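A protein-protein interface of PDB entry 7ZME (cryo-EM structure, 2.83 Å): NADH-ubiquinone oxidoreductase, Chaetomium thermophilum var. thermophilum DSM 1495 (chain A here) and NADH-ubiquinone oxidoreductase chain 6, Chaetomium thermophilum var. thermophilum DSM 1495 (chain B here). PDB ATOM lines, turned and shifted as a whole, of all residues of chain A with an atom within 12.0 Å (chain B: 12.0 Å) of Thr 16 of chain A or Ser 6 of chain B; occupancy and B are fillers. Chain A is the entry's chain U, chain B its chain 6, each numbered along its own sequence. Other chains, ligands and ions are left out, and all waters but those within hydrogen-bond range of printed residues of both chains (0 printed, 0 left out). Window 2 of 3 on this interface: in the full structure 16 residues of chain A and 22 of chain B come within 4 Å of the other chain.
N of Val 12 of chain A sits at hydrogen-bond distance from O of Leu 10 of chain B (3.0 Å).
N of Leu 8 of chain B is in hydrogen-bond range of O of Leu 14 of chain A, 3.2 Å away.
O of Ser 6 of chain B is in hydrogen-bond range of N of Thr 16 of chain A, 3.0 Å away.
The backbone carbonyl oxygen (O) of Val 12 of chain A sits close to the backbone carbonyl oxygen (O) of Leu 8 of chain B (3.4 Å).
O of Leu 14 of chain A lies close to O of Ser 6 of chain B, 3.4 Å away.
OD1 of Asp 15 of chain A lies close to O of Ser 6 of chain B (3.0 Å).
OD1 of Asp 15 of chain A is in hydrogen-bond range of OG1 of Thr 17 of chain A.
Leu 9 of chain B touches Val 12 of chain A (CA to O, 3.8 Å).
Leu 13 of chain A touches Leu 8 of chain B (CA to O, 3.6 Å).
Leu 13 of chain A touches Ile 170 of chain B (CB to CD1, 3.9 Å).
Leu 14 of chain A touches Leu 7 of chain B.
Asp 15 of chain A touches Leu 7 of chain B (OD1 to CD2, 3.6 Å).
Thr 16 of chain A touches Leu 8 of chain B.
Thr 16 of chain A touches two residues of chain B.
Of the printed residues of chain B, Asp 15 of chain A touches Ser 6 and Leu 7.
No residue of chain B comes within 4 Å of Pro 18 of chain A.
Ile 5 of chain B touches none of the printed residues of chain A.
Leu 8 of chain B touches just these residues of chain A: Val 12, Leu 13, Leu 14 and Thr 16.
Printed residues of chain B within 4 Å of Val 12 of chain A: Leu 8, Leu 9 and Leu 10.
Of the printed residues of chain A, Leu 9 of chain B touches Val 12.
Of the printed residues of chain A, Leu 10 of chain B touches Val 12 (3.0 Å).
Printed residues of chain B within 4 Å of Leu 13 of chain A: Leu 8 (3.6 Å) and Ile 170 (3.9 Å).
Of the printed residues of chain A, Ile 170 of chain B touches Leu 13 (3.9 Å).
Asp 21 of chain A touches none of the printed residues of chain B.
Ser 3 of chain B touches none of the printed residues of chain A.
The nearest printed residue of chain A that does not touch Ser 6 of chain B is Thr 17 of chain A (4.01 Å).
The nearest printed residue of chain A that does not touch Leu 10 of chain B is Leu 14 of chain A (4.5 Å).
Of the 10 printed residues of chain A, 5 touch a printed residue of chain B.
Hydrophobic or aromatic side chains of chain A within 4 Å of the printed part of chain B: Leu 13 and Leu 14.
Hydrophobic or aromatic side chains of chain B that line the printed part of chain A: Leu 7, Leu 8, Leu 9, Leu 10 and Ile 170.
Among the printed residues, no Asp or Glu carboxylate lies within 4 Å of a Lys or Arg side-chain nitrogen of the other chain.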
ATOM      1  N   VAL A  12      -4.531  -2.511   2.921  1.00  0.00           N
ATOM      2  CA  VAL A  12      -3.338  -2.465   3.805  1.00  0.00           C
ATOM      3  C   VAL A  12      -2.293  -3.423   3.223  1.00  0.00           C
ATOM      4  O   VAL A  12      -2.681  -4.522   2.803  1.00  0.00           O
ATOM      5  CB  VAL A  12      -3.746  -2.842   5.241  1.00  0.00           C
ATOM      6  CG1 VAL A  12      -2.588  -3.400   6.045  1.00  0.00           C
ATOM      7  CG2 VAL A  12      -4.413  -1.683   5.965  1.00  0.00           C
ATOM      8  N   LEU A  13      -1.032  -2.999   3.139  1.00  0.00           N
ATOM      9  CA  LEU A  13       0.059  -3.893   2.675  1.00  0.00           C
ATOM     10  C   LEU A  13       0.888  -4.280   3.899  1.00  0.00           C
ATOM     11  O   LEU A  13       1.216  -3.381   4.680  1.00  0.00           O
ATOM     12  CB  LEU A  13       0.906  -3.165   1.630  1.00  0.00           C
ATOM     13  CG  LEU A  13       1.880  -4.030   0.837  1.00  0.00           C
ATOM     14  CD1 LEU A  13       1.147  -5.131   0.086  1.00  0.00           C
ATOM     15  CD2 LEU A  13       2.678  -3.171  -0.127  1.00  0.00           C
ATOM     16  N   LEU A  14       1.175  -5.572   4.070  1.00  0.00           N
ATOM     17  CA  LEU A  14       1.973  -6.060   5.222  1.00  0.00           C
ATOM     18  C   LEU A  14       3.218  -6.773   4.698  1.00  0.00           C
ATOM     19  O   LEU A  14       3.140  -7.356   3.612  1.00  0.00           O
ATOM     20  CB  LEU A  14       1.121  -7.016   6.065  1.00  0.00           C
ATOM     21  CG  LEU A  14      -0.124  -6.418   6.711  1.00  0.00           C
ATOM     22  CD1 LEU A  14      -1.375  -6.840   5.955  1.00  0.00           C
ATOM     23  CD2 LEU A  14      -0.227  -6.841   8.164  1.00  0.00           C
ATOM     24  N   ASP A  15       4.330  -6.705   5.423  1.00  0.00           N
ATOM     25  CA  ASP A  15       5.547  -7.466   5.026  1.00  0.00           C
ATOM     26  C   ASP A  15       5.827  -8.548   6.077  1.00  0.00           C
ATOM     27  O   ASP A  15       5.942  -8.205   7.257  1.00  0.00           O
ATOM     28  CB  ASP A  15       6.743  -6.538   4.833  1.00  0.00           C
ATOM     29  CG  ASP A  15       7.481  -6.790   3.533  1.00  0.00           C
ATOM     30  OD1 ASP A  15       7.320  -7.895   2.979  1.00  0.00           O
ATOM     31  OD2 ASP A  15       8.195  -5.874   3.079  1.00  0.00           O
ATOM     32  N   THR A  16       5.941  -9.805   5.718  1.00  0.00           N
ATOM     33  CA  THR A  16       6.154 -10.837   6.765  1.00  0.00           C
ATOM     34  C   THR A  16       7.653 -11.109   6.862  1.00  0.00           C
ATOM     35  O   THR A  16       8.035 -12.002   7.623  1.00  0.00           O
ATOM     36  CB  THR A  16       5.234 -12.056   6.601  1.00  0.00           C
ATOM     37  OG1 THR A  16       5.507 -12.750   5.387  1.00  0.00           O
ATOM     38  CG2 THR A  16       3.770 -11.696   6.683  1.00  0.00           C
ATOM     39  N   THR A  17       8.452 -10.337   6.078  1.00  0.00           N
ATOM     40  CA  THR A  17       9.929 -10.459   6.144  1.00  0.00           C
ATOM     41  C   THR A  17      10.455  -9.943   7.493  1.00  0.00           C
ATOM     42  O   THR A  17      10.166  -8.785   7.804  1.00  0.00           O
ATOM     43  CB  THR A  17      10.577  -9.667   5.011  1.00  0.00           C
ATOM     44  OG1 THR A  17       9.729  -9.768   3.870  1.00  0.00           O
ATOM     45  CG2 THR A  17      11.971 -10.152   4.681  1.00  0.00           C
ATOM     46  N   PRO A  18      11.206 -10.726   8.310  1.00  0.00           N
ATOM     47  CA  PRO A  18      11.743 -10.255   9.576  1.00  0.00           C
ATOM     48  C   PRO A  18      13.054  -9.474   9.429  1.00  0.00           C
ATOM     49  O   PRO A  18      13.739  -9.684   8.454  1.00  0.00           O
ATOM     50  CB  PRO A  18      11.971 -11.545  10.376  1.00  0.00           C
ATOM     51  CG  PRO A  18      11.417 -12.658   9.531  1.00  0.00           C
ATOM     52  CD  PRO A  18      11.580 -12.142   8.124  1.00  0.00           C
ATOM     53  N   LEU A  19      13.385  -8.634  10.409  1.00  0.00           N
ATOM     54  CA  LEU A  19      14.646  -7.860  10.384  1.00  0.00           C
ATOM     55  C   LEU A  19      15.797  -8.859  10.390  1.00  0.00           C
ATOM     56  O   LEU A  19      15.659  -9.887  11.078  1.00  0.00           O
ATOM     57  CB  LEU A  19      14.709  -6.978  11.633  1.00  0.00           C
ATOM     58  CG  LEU A  19      14.323  -5.512  11.463  1.00  0.00           C
ATOM     59  CD1 LEU A  19      14.159  -4.834  12.813  1.00  0.00           C
ATOM     60  CD2 LEU A  19      15.346  -4.772  10.621  1.00  0.00           C
ATOM     61  N   PRO A  20      16.925  -8.619   9.676  1.00  0.00           N
ATOM     62  CA  PRO A  20      18.002  -9.623   9.579  1.00  0.00           C
ATOM     63  C   PRO A  20      18.730  -9.973  10.885  1.00  0.00           C
ATOM     64  O   PRO A  20      18.748  -9.124  11.750  1.00  0.00           O
ATOM     65  CB  PRO A  20      18.969  -8.946   8.609  1.00  0.00           C
ATOM     66  CG  PRO A  20      18.104  -8.004   7.820  1.00  0.00           C
ATOM     67  CD  PRO A  20      17.184  -7.436   8.871  1.00  0.00           C
ATOM     68  N   ASP A  21      19.311 -11.176  11.018  1.00  0.00           N
ATOM     69  CA  ASP A  21      19.950 -11.633  12.246  1.00  0.00           C
ATOM     70  C   ASP A  21      21.031 -10.678  12.738  1.00  0.00           C
ATOM     71  O   ASP A  21      21.408 -10.746  13.912  1.00  0.00           O
ATOM     72  CB  ASP A  21      20.549 -13.022  12.039  1.00  0.00           C
ATOM     73  CG  ASP A  21      19.496 -14.108  11.986  1.00  0.00           C
ATOM     74  OD1 ASP A  21      18.357 -13.852  12.428  1.00  0.00           O
ATOM     75  OD2 ASP A  21      19.808 -15.218  11.506  1.00  0.00           O
ATOM     76  N   SER B   3       5.727 -21.967  -0.837  1.00  0.00           N
ATOM     77  CA  SER B   3       6.957 -21.293  -0.443  1.00  0.00           C
ATOM     78  C   SER B   3       6.671 -20.182   0.562  1.00  0.00           C
ATOM     79  O   SER B   3       6.384 -20.448   1.729  1.00  0.00           O
ATOM     80  CB  SER B   3       7.673 -20.724  -1.670  1.00  0.00           C
ATOM     81  N   GLN B   4       6.752 -18.934   0.101  1.00  0.00           N
ATOM     82  CA  GLN B   4       6.506 -17.788   0.967  1.00  0.00           C
ATOM     83  C   GLN B   4       6.124 -16.557   0.153  1.00  0.00           C
ATOM     84  O   GLN B   4       6.947 -16.026  -0.600  1.00  0.00           O
ATOM     85  CB  GLN B   4       7.736 -17.492   1.826  1.00  0.00           C
ATOM     86  N   ILE B   5       4.886 -16.082   0.309  1.00  0.00           N
ATOM     87  CA  ILE B   5       4.493 -14.815  -0.380  1.00  0.00           C
ATOM     88  C   ILE B   5       5.268 -13.677   0.281  1.00  0.00           C
ATOM     89  O   ILE B   5       6.142 -13.110  -0.407  1.00  0.00           O
ATOM     90  CB  ILE B   5       2.973 -14.587  -0.277  1.00  0.00           C
ATOM     91  N   SER B   6       4.898 -13.310   1.512  1.00  0.00           N
ATOM     92  CA  SER B   6       5.583 -12.252   2.307  1.00  0.00           C
ATOM     93  C   SER B   6       5.028 -10.860   1.999  1.00  0.00           C
ATOM     94  O   SER B   6       5.221  -9.969   2.835  1.00  0.00           O
ATOM     95  CB  SER B   6       7.090 -12.317   2.253  1.00  0.00           C
ATOM     96  OG  SER B   6       7.566 -13.490   2.892  1.00  0.00           O
ATOM     97  N   LEU B   7       4.298 -10.697   0.901  1.00  0.00           N
ATOM     98  CA  LEU B   7       3.648  -9.390   0.620  1.00  0.00           C
ATOM     99  C   LEU B   7       2.148  -9.647   0.616  1.00  0.00           C
ATOM    100  O   LEU B   7       1.674 -10.310  -0.317  1.00  0.00           O
ATOM    101  CB  LEU B   7       4.147  -8.794  -0.700  1.00  0.00           C
ATOM    102  CG  LEU B   7       5.300  -7.803  -0.576  1.00  0.00           C
ATOM    103  CD1 LEU B   7       5.555  -7.116  -1.905  1.00  0.00           C
ATOM    104  CD2 LEU B   7       5.012  -6.774   0.505  1.00  0.00           C
ATOM    105  N   LEU B   8       1.436  -9.149   1.626  1.00  0.00           N
ATOM    106  CA  LEU B   8       0.009  -9.527   1.741  1.00  0.00           C
ATOM    107  C   LEU B   8      -0.905  -8.330   1.490  1.00  0.00           C
ATOM    108  O   LEU B   8      -0.775  -7.327   2.207  1.00  0.00           O
ATOM    109  CB  LEU B   8      -0.213 -10.126   3.129  1.00  0.00           C
ATOM    110  CG  LEU B   8       0.860 -11.108   3.597  1.00  0.00           C
ATOM    111  CD1 LEU B   8       0.804 -11.305   5.102  1.00  0.00           C
ATOM    112  CD2 LEU B   8       0.735 -12.438   2.874  1.00  0.00           C
ATOM    113  N   LEU B   9      -1.817  -8.478   0.467  1.00  0.00           N
ATOM    114  CA  LEU B   9      -2.776  -7.375   0.244  1.00  0.00           C
ATOM    115  C   LEU B   9      -4.013  -7.705   1.068  1.00  0.00           C
ATOM    116  O   LEU B   9      -4.335  -8.888   1.204  1.00  0.00           O
ATOM    117  CB  LEU B   9      -3.079  -7.178  -1.243  1.00  0.00           C
ATOM    118  CG  LEU B   9      -3.669  -5.819  -1.615  1.00  0.00           C
ATOM    119  CD1 LEU B   9      -2.826  -4.686  -1.054  1.00  0.00           C
ATOM    120  CD2 LEU B   9      -3.798  -5.687  -3.124  1.00  0.00           C
ATOM    121  N   LEU B  10      -4.645  -6.693   1.628  1.00  0.00           N
ATOM    122  CA  LEU B  10      -5.810  -6.888   2.469  1.00  0.00           C
ATOM    123  C   LEU B  10      -6.755  -5.715   2.287  1.00  0.00           C
ATOM    124  O   LEU B  10      -6.353  -4.635   1.857  1.00  0.00           O
ATOM    125  CB  LEU B  10      -5.392  -7.033   3.935  1.00  0.00           C
ATOM    126  CG  LEU B  10      -6.396  -7.611   4.921  1.00  0.00           C
ATOM    127  CD1 LEU B  10      -6.379  -9.113   4.866  1.00  0.00           C
ATOM    128  CD2 LEU B  10      -6.047  -7.125   6.309  1.00  0.00           C
ATOM    129  N   ILE B 170       1.631   4.403  -1.206  1.00  0.00           N
ATOM    130  CA  ILE B 170       1.789   3.746   0.124  1.00  0.00           C
ATOM    131  C   ILE B 170       2.031   4.825   1.184  1.00  0.00           C
ATOM    132  O   ILE B 170       2.850   5.718   0.937  1.00  0.00           O
ATOM    133  CB  ILE B 170       2.876   2.651   0.073  1.00  0.00           C
ATOM    134  CG1 ILE B 170       2.795   1.706   1.273  1.00  0.00           C
ATOM    135  CG2 ILE B 170       4.269   3.223  -0.113  1.00  0.00           C
ATOM    136  CD1 ILE B 170       1.715   0.667   1.154  1.00  0.00           C
